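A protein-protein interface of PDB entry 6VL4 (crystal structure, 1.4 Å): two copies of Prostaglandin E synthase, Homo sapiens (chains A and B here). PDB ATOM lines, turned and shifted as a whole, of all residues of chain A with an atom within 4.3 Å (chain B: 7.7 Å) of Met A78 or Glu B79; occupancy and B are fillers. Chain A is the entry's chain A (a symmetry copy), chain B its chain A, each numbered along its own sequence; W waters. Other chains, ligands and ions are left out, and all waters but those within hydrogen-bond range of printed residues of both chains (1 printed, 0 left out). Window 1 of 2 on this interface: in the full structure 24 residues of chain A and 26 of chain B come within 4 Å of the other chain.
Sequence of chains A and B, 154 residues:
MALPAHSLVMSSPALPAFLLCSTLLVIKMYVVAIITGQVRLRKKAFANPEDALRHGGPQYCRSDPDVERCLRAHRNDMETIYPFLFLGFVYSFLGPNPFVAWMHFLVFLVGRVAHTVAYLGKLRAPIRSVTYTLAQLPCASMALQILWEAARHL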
ATOM      1  N   MET A  29      10.383 -21.506  -6.858  1.00  0.00           N
ATOM      2  CA  MET A  29       9.624 -20.299  -6.566  1.00  0.00           C
ATOM      3  C   MET A  29      10.532 -19.069  -6.614  1.00  0.00           C
ATOM      4  O   MET A  29      10.125 -18.019  -7.109  1.00  0.00           O
ATOM      5  CB  MET A  29       8.913 -20.388  -5.213  1.00  0.00           C
ATOM      6  CG  MET A  29       7.714 -21.318  -5.244  1.00  0.00           C
ATOM      7  SD  MET A  29       6.734 -21.338  -3.721  1.00  0.00           S
ATOM      8  CE  MET A  29       6.217 -19.627  -3.637  1.00  0.00           C
ATOM      9  N   HIS A  74       3.334 -17.093  -9.420  1.00  0.00           N
ATOM     10  CA  HIS A  74       3.894 -17.078  -8.077  1.00  0.00           C
ATOM     11  C   HIS A  74       2.792 -17.279  -7.039  1.00  0.00           C
ATOM     12  O   HIS A  74       2.981 -18.012  -6.067  1.00  0.00           O
ATOM     13  CB  HIS A  74       4.680 -15.783  -7.828  1.00  0.00           C
ATOM     14  CG  HIS A  74       5.698 -15.878  -6.738  1.00  0.00           C
ATOM     15  ND1 HIS A  74       6.713 -14.954  -6.608  1.00  0.00           N
ATOM     16  CD2 HIS A  74       5.882 -16.779  -5.745  1.00  0.00           C
ATOM     17  CE1 HIS A  74       7.468 -15.268  -5.573  1.00  0.00           C
ATOM     18  NE2 HIS A  74       6.981 -16.387  -5.029  1.00  0.00           N
ATOM     19  N   ARG A  75       1.632 -16.649  -7.249  1.00  0.00           N
ATOM     20  CA  ARG A  75       0.525 -16.786  -6.319  1.00  0.00           C
ATOM     21  C   ARG A  75       0.034 -18.234  -6.268  1.00  0.00           C
ATOM     22  O   ARG A  75      -0.209 -18.771  -5.186  1.00  0.00           O
ATOM     23  CB  ARG A  75      -0.604 -15.811  -6.656  1.00  0.00           C
ATOM     24  CG  ARG A  75      -1.719 -15.824  -5.622  1.00  0.00           C
ATOM     25  CD  ARG A  75      -2.849 -14.867  -5.902  1.00  0.00           C
ATOM     26  NE  ARG A  75      -3.949 -15.299  -5.059  1.00  0.00           N
ATOM     27  CZ  ARG A  75      -4.958 -14.539  -4.658  1.00  0.00           C
ATOM     28  NH1 ARG A  75      -5.958 -15.094  -4.001  1.00  0.00           N
ATOM     29  NH2 ARG A  75      -4.977 -13.241  -4.915  1.00  0.00           N
ATOM     30  N   ASN A  76      -0.121 -18.861  -7.439  1.00  0.00           N
ATOM     31  CA  ASN A  76      -0.586 -20.238  -7.508  1.00  0.00           C
ATOM     32  C   ASN A  76       0.403 -21.164  -6.800  1.00  0.00           C
ATOM     33  O   ASN A  76      -0.014 -22.102  -6.119  1.00  0.00           O
ATOM     34  CB  ASN A  76      -0.923 -20.667  -8.938  1.00  0.00           C
ATOM     35  CG  ASN A  76      -1.585 -22.029  -8.993  1.00  0.00           C
ATOM     36  OD1 ASN A  76      -0.908 -23.046  -9.109  1.00  0.00           O
ATOM     37  ND2 ASN A  76      -2.905 -22.060  -8.914  1.00  0.00           N
ATOM     38  N   ASP A  77       1.702 -20.876  -6.956  1.00  0.00           N
ATOM     39  CA  ASP A  77       2.757 -21.582  -6.242  1.00  0.00           C
ATOM     40  C   ASP A  77       2.519 -21.504  -4.733  1.00  0.00           C
ATOM     41  O   ASP A  77       2.599 -22.519  -4.045  1.00  0.00           O
ATOM     42  CB  ASP A  77       4.142 -21.012  -6.562  1.00  0.00           C
ATOM     43  CG  ASP A  77       4.719 -21.358  -7.926  1.00  0.00           C
ATOM     44  OD1 ASP A  77       4.096 -22.152  -8.668  1.00  0.00           O
ATOM     45  OD2 ASP A  77       5.801 -20.823  -8.234  1.00  0.00           O
ATOM     46  N   MET A  78       2.220 -20.301  -4.222  1.00  0.00           N
ATOM     47  CA  MET A  78       2.043 -20.104  -2.788  1.00  0.00           C
ATOM     48  C   MET A  78       0.807 -20.855  -2.291  1.00  0.00           C
ATOM     49  O   MET A  78       0.795 -21.344  -1.161  1.00  0.00           O
ATOM     50  CB  MET A  78       1.911 -18.622  -2.426  1.00  0.00           C
ATOM     51  CG  MET A  78       3.157 -17.808  -2.709  1.00  0.00           C
ATOM     52  SD  MET A  78       3.247 -16.260  -1.774  1.00  0.00           S
ATOM     53  CE  MET A  78       1.741 -15.435  -2.288  1.00  0.00           C
ATOM     54  N   GLU A  79      -0.226 -20.950  -3.142  1.00  0.00           N
ATOM     55  CA  GLU A  79      -1.479 -21.609  -2.801  1.00  0.00           C
ATOM     56  C   GLU A  79      -1.315 -23.128  -2.731  1.00  0.00           C
ATOM     57  O   GLU A  79      -2.133 -23.792  -2.094  1.00  0.00           O
ATOM     58  CB  GLU A  79      -2.556 -21.281  -3.836  1.00  0.00           C
ATOM     59  CG  GLU A  79      -3.049 -19.847  -3.788  1.00  0.00           C
ATOM     60  CD  GLU A  79      -3.946 -19.438  -4.945  1.00  0.00           C
ATOM     61  OE1 GLU A  79      -4.231 -20.287  -5.815  1.00  0.00           O
ATOM     62  OE2 GLU A  79      -4.357 -18.264  -4.972  1.00  0.00           O
ATOM     63  N   THR A  80      -0.287 -23.670  -3.401  1.00  0.00           N
ATOM     64  CA  THR A  80      -0.172 -25.110  -3.603  1.00  0.00           C
ATOM     65  C   THR A  80       1.070 -25.681  -2.920  1.00  0.00           C
ATOM     66  O   THR A  80       0.986 -26.728  -2.277  1.00  0.00           O
ATOM     67  CB  THR A  80      -0.232 -25.483  -5.091  1.00  0.00           C
ATOM     68  OG1 THR A  80       0.823 -24.805  -5.775  1.00  0.00           O
ATOM     69  CG2 THR A  80      -1.563 -25.148  -5.727  1.00  0.00           C
ATOM     70  N   TYR A  82       3.021 -24.295  -0.512  1.00  0.00           N
ATOM     71  CA  TYR A  82       3.069 -24.080   0.928  1.00  0.00           C
ATOM     72  C   TYR A  82       2.289 -25.171   1.669  1.00  0.00           C
ATOM     73  O   TYR A  82       2.822 -25.745   2.620  1.00  0.00           O
ATOM     74  CB  TYR A  82       2.658 -22.651   1.307  1.00  0.00           C
ATOM     75  CG  TYR A  82       3.562 -21.524   0.860  1.00  0.00           C
ATOM     76  CD1 TYR A  82       4.819 -21.743   0.311  1.00  0.00           C
ATOM     77  CD2 TYR A  82       3.156 -20.207   1.028  1.00  0.00           C
ATOM     78  CE1 TYR A  82       5.632 -20.689  -0.086  1.00  0.00           C
ATOM     79  CE2 TYR A  82       3.952 -19.142   0.634  1.00  0.00           C
ATOM     80  CZ  TYR A  82       5.198 -19.384   0.086  1.00  0.00           C
ATOM     81  OH  TYR A  82       5.989 -18.339  -0.287  1.00  0.00           O
ATOM     82  N   PRO A  83       1.025 -25.501   1.290  1.00  0.00           N
ATOM     83  CA  PRO A  83       0.334 -26.666   1.849  1.00  0.00           C
ATOM     84  C   PRO A  83       1.131 -27.965   1.750  1.00  0.00           C
ATOM     85  O   PRO A  83       1.127 -28.746   2.694  1.00  0.00           O
ATOM     86  CB  PRO A  83      -0.969 -26.738   1.040  1.00  0.00           C
ATOM     87  CG  PRO A  83      -1.235 -25.293   0.691  1.00  0.00           C
ATOM     88  CD  PRO A  83       0.140 -24.733   0.391  1.00  0.00           C
ATOM     89  N   MET B  29       4.407  -9.485  10.401  1.00  0.00           N
ATOM     90  CA  MET B  29       3.407  -9.623   9.353  1.00  0.00           C
ATOM     91  C   MET B  29       2.026  -9.221   9.872  1.00  0.00           C
ATOM     92  O   MET B  29       1.258  -8.582   9.153  1.00  0.00           O
ATOM     93  CB  MET B  29       3.375 -11.044   8.783  1.00  0.00           C
ATOM     94  CG  MET B  29       4.568 -11.346   7.896  1.00  0.00           C
ATOM     95  SD  MET B  29       4.501 -12.952   7.062  1.00  0.00           S
ATOM     96  CE  MET B  29       3.012 -12.759   6.088  1.00  0.00           C
ATOM     97  N   ARG B  72       0.993  -5.062  -1.211  1.00  0.00           N
ATOM     98  CA  ARG B  72       2.215  -5.514  -1.861  1.00  0.00           C
ATOM     99  C   ARG B  72       3.268  -5.914  -0.828  1.00  0.00           C
ATOM    100  O   ARG B  72       3.963  -6.915  -1.019  1.00  0.00           O
ATOM    101  CB  ARG B  72       2.772  -4.457  -2.819  1.00  0.00           C
ATOM    102  CG  ARG B  72       2.017  -4.341  -4.136  1.00  0.00           C
ATOM    103  CD  ARG B  72       2.743  -3.501  -5.172  1.00  0.00           C
ATOM    104  NE  ARG B  72       3.052  -2.143  -4.738  1.00  0.00           N
ATOM    105  CZ  ARG B  72       2.206  -1.114  -4.782  1.00  0.00           C
ATOM    106  NH1 ARG B  72       0.980  -1.273  -5.254  1.00  0.00           N
ATOM    107  NH2 ARG B  72       2.596   0.074  -4.355  1.00  0.00           N
ATOM    108  N   ALA B  73       3.380  -5.137   0.257  1.00  0.00           N
ATOM    109  CA  ALA B  73       4.323  -5.432   1.329  1.00  0.00           C
ATOM    110  C   ALA B  73       3.979  -6.769   1.981  1.00  0.00           C
ATOM    111  O   ALA B  73       4.871  -7.589   2.201  1.00  0.00           O
ATOM    112  CB  ALA B  73       4.359  -4.304   2.332  1.00  0.00           C
ATOM    113  N   HIS B  74       2.686  -6.988   2.244  1.00  0.00           N
ATOM    114  CA  HIS B  74       2.223  -8.222   2.862  1.00  0.00           C
ATOM    115  C   HIS B  74       2.468  -9.407   1.930  1.00  0.00           C
ATOM    116  O   HIS B  74       2.888 -10.475   2.380  1.00  0.00           O
ATOM    117  CB  HIS B  74       0.747  -8.111   3.264  1.00  0.00           C
ATOM    118  CG  HIS B  74       0.324  -9.065   4.336  1.00  0.00           C
ATOM    119  ND1 HIS B  74      -0.838  -8.883   5.055  1.00  0.00           N
ATOM    120  CD2 HIS B  74       0.899 -10.186   4.829  1.00  0.00           C
ATOM    121  CE1 HIS B  74      -0.973  -9.858   5.932  1.00  0.00           C
ATOM    122  NE2 HIS B  74       0.083 -10.669   5.817  1.00  0.00           N
ATOM    123  N   ARG B  75       2.228  -9.221   0.629  1.00  0.00           N
ATOM    124  CA  ARG B  75       2.437 -10.289  -0.333  1.00  0.00           C
ATOM    125  C   ARG B  75       3.914 -10.686  -0.392  1.00  0.00           C
ATOM    126  O   ARG B  75       4.238 -11.874  -0.402  1.00  0.00           O
ATOM    127  CB  ARG B  75       1.894  -9.908  -1.711  1.00  0.00           C
ATOM    128  CG  ARG B  75       1.966 -11.054  -2.708  1.00  0.00           C
ATOM    129  CD  ARG B  75       1.426 -10.730  -4.077  1.00  0.00           C
ATOM    130  NE  ARG B  75       1.930 -11.771  -4.955  1.00  0.00           N
ATOM    131  CZ  ARG B  75       1.391 -12.135  -6.110  1.00  0.00           C
ATOM    132  NH1 ARG B  75       2.027 -13.007  -6.868  1.00  0.00           N
ATOM    133  NH2 ARG B  75       0.236 -11.630  -6.510  1.00  0.00           N
ATOM    134  N   ASN B  76       4.806  -9.690  -0.437  1.00  0.00           N
ATOM    135  CA  ASN B  76       6.236  -9.953  -0.498  1.00  0.00           C
ATOM    136  C   ASN B  76       6.688 -10.703   0.755  1.00  0.00           C
ATOM    137  O   ASN B  76       7.524 -11.603   0.665  1.00  0.00           O
ATOM    138  CB  ASN B  76       7.048  -8.689  -0.790  1.00  0.00           C
ATOM    139  CG  ASN B  76       8.511  -8.987  -1.043  1.00  0.00           C
ATOM    140  OD1 ASN B  76       9.314  -8.993  -0.116  1.00  0.00           O
ATOM    141  ND2 ASN B  76       8.868  -9.233  -2.293  1.00  0.00           N
ATOM    142  N   ASP B  77       6.111 -10.336   1.908  1.00  0.00           N
ATOM    143  CA  ASP B  77       6.337 -11.039   3.162  1.00  0.00           C
ATOM    144  C   ASP B  77       5.988 -12.520   3.009  1.00  0.00           C
ATOM    145  O   ASP B  77       6.765 -13.380   3.416  1.00  0.00           O
ATOM    146  CB  ASP B  77       5.512 -10.444   4.307  1.00  0.00           C
ATOM    147  CG  ASP B  77       5.991  -9.115   4.869  1.00  0.00           C
ATOM    148  OD1 ASP B  77       7.067  -8.628   4.450  1.00  0.00           O
ATOM    149  OD2 ASP B  77       5.275  -8.577   5.735  1.00  0.00           O
ATOM    150  N   MET B  78       4.822 -12.816   2.416  1.00  0.00           N
ATOM    151  CA  MET B  78       4.362 -14.193   2.282  1.00  0.00           C
ATOM    152  C   MET B  78       5.279 -14.977   1.342  1.00  0.00           C
ATOM    153  O   MET B  78       5.488 -16.174   1.541  1.00  0.00           O
ATOM    154  CB  MET B  78       2.924 -14.268   1.760  1.00  0.00           C
ATOM    155  CG  MET B  78       1.898 -13.678   2.705  1.00  0.00           C
ATOM    156  SD  MET B  78       0.211 -14.269   2.415  1.00  0.00           S
ATOM    157  CE  MET B  78      -0.054 -13.792   0.706  1.00  0.00           C
ATOM    158  N   GLU B  79       5.830 -14.296   0.327  1.00  0.00           N
ATOM    159  CA  GLU B  79       6.700 -14.913  -0.665  1.00  0.00           C
ATOM    160  C   GLU B  79       8.067 -15.262  -0.075  1.00  0.00           C
ATOM    161  O   GLU B  79       8.762 -16.113  -0.630  1.00  0.00           O
ATOM    162  CB  GLU B  79       6.906 -13.974  -1.855  1.00  0.00           C
ATOM    163  CG  GLU B  79       5.678 -13.797  -2.729  1.00  0.00           C
ATOM    164  CD  GLU B  79       5.789 -12.702  -3.777  1.00  0.00           C
ATOM    165  OE1 GLU B  79       6.856 -12.059  -3.865  1.00  0.00           O
ATOM    166  OE2 GLU B  79       4.801 -12.494  -4.503  1.00  0.00           O
ATOM    167  N   THR B  80       8.457 -14.590   1.020  1.00  0.00           N
ATOM    168  CA  THR B  80       9.824 -14.664   1.523  1.00  0.00           C
ATOM    169  C   THR B  80       9.882 -15.289   2.917  1.00  0.00           C
ATOM    170  O   THR B  80      10.742 -16.132   3.173  1.00  0.00           O
ATOM    171  CB  THR B  80      10.523 -13.299   1.476  1.00  0.00           C
ATOM    172  OG1 THR B  80       9.765 -12.370   2.250  1.00  0.00           O
ATOM    173  CG2 THR B  80      10.700 -12.778   0.067  1.00  0.00           C
ATOM    174  N   ILE B  81       8.981 -14.867   3.812  1.00  0.00           N
ATOM    175  CA  ILE B  81       9.033 -15.290   5.206  1.00  0.00           C
ATOM    176  C   ILE B  81       8.553 -16.737   5.325  1.00  0.00           C
ATOM    177  O   ILE B  81       9.123 -17.506   6.096  1.00  0.00           O
ATOM    178  CB  ILE B  81       8.273 -14.311   6.125  1.00  0.00           C
ATOM    179  CG1 ILE B  81       8.957 -12.940   6.145  1.00  0.00           C
ATOM    180  CG2 ILE B  81       8.106 -14.882   7.531  1.00  0.00           C
ATOM    181  CD1 ILE B  81       8.137 -11.831   6.760  1.00  0.00           C
ATOM    182  N   TYR B  82       7.530 -17.115   4.547  1.00  0.00           N
ATOM    183  CA  TYR B  82       6.992 -18.467   4.624  1.00  0.00           C
ATOM    184  C   TYR B  82       8.054 -19.500   4.232  1.00  0.00           C
ATOM    185  O   TYR B  82       8.240 -20.473   4.965  1.00  0.00           O
ATOM    186  CB  TYR B  82       5.673 -18.603   3.851  1.00  0.00           C
ATOM    187  CG  TYR B  82       4.479 -17.834   4.369  1.00  0.00           C
ATOM    188  CD1 TYR B  82       4.479 -17.188   5.600  1.00  0.00           C
ATOM    189  CD2 TYR B  82       3.311 -17.787   3.620  1.00  0.00           C
ATOM    190  CE1 TYR B  82       3.365 -16.494   6.055  1.00  0.00           C
ATOM    191  CE2 TYR B  82       2.191 -17.095   4.056  1.00  0.00           C
ATOM    192  CZ  TYR B  82       2.216 -16.456   5.282  1.00  0.00           C
ATOM    193  OH  TYR B  82       1.111 -15.789   5.721  1.00  0.00           O
ATOM    194  N   PRO B  83       8.780 -19.352   3.092  1.00  0.00           N
ATOM    195  CA  PRO B  83       9.928 -20.212   2.795  1.00  0.00           C
ATOM    196  C   PRO B  83      10.962 -20.275   3.918  1.00  0.00           C
ATOM    197  O   PRO B  83      11.484 -21.348   4.195  1.00  0.00           O
ATOM    198  CB  PRO B  83      10.519 -19.600   1.516  1.00  0.00           C
ATOM    199  CG  PRO B  83       9.311 -19.008   0.831  1.00  0.00           C
ATOM    200  CD  PRO B  83       8.492 -18.435   1.970  1.00  0.00           C
ATOM    201  N   PHE B  84      11.231 -19.136   4.570  1.00  0.00           N
ATOM    202  CA  PHE B  84      12.184 -19.081   5.672  1.00  0.00           C
ATOM    203  C   PHE B  84      11.717 -19.951   6.837  1.00  0.00           C
ATOM    204  O   PHE B  84      12.538 -20.639   7.450  1.00  0.00           O
ATOM    205  CB  PHE B  84      12.425 -17.641   6.130  1.00  0.00           C
ATOM    206  CG  PHE B  84      13.283 -17.497   7.364  1.00  0.00           C
ATOM    207  CD1 PHE B  84      14.669 -17.452   7.269  1.00  0.00           C
ATOM    208  CD2 PHE B  84      12.704 -17.387   8.622  1.00  0.00           C
ATOM    209  CE1 PHE B  84      15.453 -17.308   8.406  1.00  0.00           C
ATOM    210  CE2 PHE B  84      13.487 -17.249   9.760  1.00  0.00           C
ATOM    211  CZ  PHE B  84      14.862 -17.211   9.649  1.00  0.00           C
ATOM    212  N   PHE B 108      18.356 -12.314   7.903  1.00  0.00           N
ATOM    213  CA  PHE B 108      16.996 -12.407   7.397  1.00  0.00           C
ATOM    214  C   PHE B 108      16.063 -11.483   8.177  1.00  0.00           C
ATOM    215  O   PHE B 108      15.291 -10.751   7.566  1.00  0.00           O
ATOM    216  CB  PHE B 108      16.479 -13.848   7.354  1.00  0.00           C
ATOM    217  CG  PHE B 108      15.165 -13.968   6.626  1.00  0.00           C
ATOM    218  CD1 PHE B 108      15.112 -13.886   5.242  1.00  0.00           C
ATOM    219  CD2 PHE B 108      13.972 -14.111   7.321  1.00  0.00           C
ATOM    220  CE1 PHE B 108      13.902 -13.972   4.569  1.00  0.00           C
ATOM    221  CE2 PHE B 108      12.762 -14.207   6.648  1.00  0.00           C
ATOM    222  CZ  PHE B 108      12.730 -14.145   5.273  1.00  0.00           C
ATOM    223  N   ARG B 112      14.342  -8.191   6.561  1.00  0.00           N
ATOM    224  CA  ARG B 112      12.898  -8.202   6.371  1.00  0.00           C
ATOM    225  C   ARG B 112      12.224  -7.034   7.090  1.00  0.00           C
ATOM    226  O   ARG B 112      11.265  -6.465   6.567  1.00  0.00           O
ATOM    227  CB  ARG B 112      12.295  -9.545   6.784  1.00  0.00           C
ATOM    228  CG  ARG B 112      12.568 -10.686   5.812  1.00  0.00           C
ATOM    229  CD  ARG B 112      12.365 -10.413   4.330  1.00  0.00           C
ATOM    230  NE  ARG B 112      11.038  -9.885   4.038  1.00  0.00           N
ATOM    231  CZ  ARG B 112      10.618  -9.507   2.836  1.00  0.00           C
ATOM    232  NH1 ARG B 112      11.417  -9.598   1.786  1.00  0.00           N
ATOM    233  NH2 ARG B 112       9.391  -9.039   2.692  1.00  0.00           N
ATOM    234  N   TYR B 132      15.411  -6.713   0.125  1.00  0.00           N
ATOM    235  CA  TYR B 132      14.752  -7.911  -0.376  1.00  0.00           C
ATOM    236  C   TYR B 132      15.805  -8.933  -0.802  1.00  0.00           C
ATOM    237  O   TYR B 132      15.790 -10.069  -0.326  1.00  0.00           O
ATOM    238  CB  TYR B 132      13.758  -7.504  -1.470  1.00  0.00           C
ATOM    239  CG  TYR B 132      13.142  -8.566  -2.350  1.00  0.00           C
ATOM    240  CD1 TYR B 132      12.774  -9.821  -1.876  1.00  0.00           C
ATOM    241  CD2 TYR B 132      12.849  -8.271  -3.674  1.00  0.00           C
ATOM    242  CE1 TYR B 132      12.185 -10.763  -2.710  1.00  0.00           C
ATOM    243  CE2 TYR B 132      12.256  -9.196  -4.518  1.00  0.00           C
ATOM    244  CZ  TYR B 132      11.920 -10.448  -4.033  1.00  0.00           C
ATOM    245  OH  TYR B 132      11.337 -11.357  -4.869  1.00  0.00           O
ATOM    246  N   GLN B 136      17.237 -12.567   1.010  1.00  0.00           N
ATOM    247  CA  GLN B 136      17.076 -13.814   0.277  1.00  0.00           C
ATOM    248  C   GLN B 136      18.348 -14.661   0.332  1.00  0.00           C
ATOM    249  O   GLN B 136      18.274 -15.880   0.175  1.00  0.00           O
ATOM    250  CB  GLN B 136      16.636 -13.577  -1.172  1.00  0.00           C
ATOM    251  CG  GLN B 136      15.199 -13.093  -1.328  1.00  0.00           C
ATOM    252  CD  GLN B 136      14.164 -13.984  -0.682  1.00  0.00           C
ATOM    253  OE1 GLN B 136      13.924 -13.921   0.521  1.00  0.00           O
ATOM    254  NE2 GLN B 136      13.526 -14.812  -1.494  1.00  0.00           N
HETATM  255  O   HOH W   1       3.259 -14.622  -5.007  1.00  0.00           O
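Among the printed residues, merely in contact across the chains: His A74 with Arg B75 (3.96 Å), His A74 with Glu B79 (3.6 Å), Arg A75 with Arg B75 (3.7 Å), Met A78 with Met B78 (3.9 Å), Met A78 with Glu B79 (3.6 Å), Tyr A82 with Glu B79 (3.5 Å), Tyr A82 with Tyr B82 (3.3 Å) and Tyr A82 with Pro B83 (3.4 Å).
The side-chain hydroxyl (OH) of Tyr A82 is in hydrogen-bond range of the backbone carbonyl oxygen (O) of Met B78 (2.9 Å).
Met A78 touches its own counterpart, Met B78. Met A78 touches Glu B79, but with the chains exchanged Glu A79 does not touch Met B78 (8.1 Å). Tyr A82 touches Met B78, but with the chains exchanged Met A78 does not touch Tyr B82 (5.6 Å). Tyr A82 touches its own counterpart, Tyr B82. Positions printed for both chains: 29, 74, 75, 76, 77, 78, 79, 80, 82 and 83.
Water W1 lies within hydrogen-bond range of OE2 of Glu B79, NH1 of Arg B75, N of Arg A75 and SD of Met A78.
Of the printed residues of chain B, His A74 touches Arg B75 (3.96 Å) and Glu B79 (3.6 Å). Of chain B, only Met B78 and Glu B79 come within 4 Å of Met A78. Of the printed residues of chain B, Tyr A82 touches Met B78 (2.9 Å), Glu B79 (3.5 Å), Tyr B82 (3.3 Å) and Pro B83 (3.4 Å). Pro A83 touches none of the printed residues of chain B. Of the printed residues of chain A, Met B78 touches Met A78 (3.9 Å) and Tyr A82 (2.9 Å). Printed residues of chain A within 4 Å of Tyr B82: Tyr A82 (3.3 Å). Of the printed residues of chain A, Pro B83 touches Tyr A82. Phe B84 touches none of the printed residues of chain A.
Of the 10 printed residues of chain A, 4 touch a printed residue of chain B. Hydrophobic or aromatic side chains of chain B within 4 Å of the printed part of chain A: Met B78, Tyr B82 and Pro B83. Among the printed residues, 9 pairs touch across the chains. Among the printed residues, no Asp or Glu carboxylate lies within 4 Å of a Lys or Arg side-chain nitrogen of the other chain.
NE of Arg A75 is in salt-bridge range of OE2 of Glu A79 (3.0 Å). The guanidinium group (NE) of Arg B75 lies within salt-bridge range of the side-chain carboxylate (OE2) of Glu B79, 3.0 Å away. The side-chain sulfur (SD) of Met B78 sits at hydrogen-bond distance from the side-chain hydroxyl (OH) of Tyr B82 (3.7 Å). The side-chain sulfur (SD) of Met A78 lies within hydrogen-bond range of the side-chain hydroxyl (OH) of Tyr A82, 3.7 Å away.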
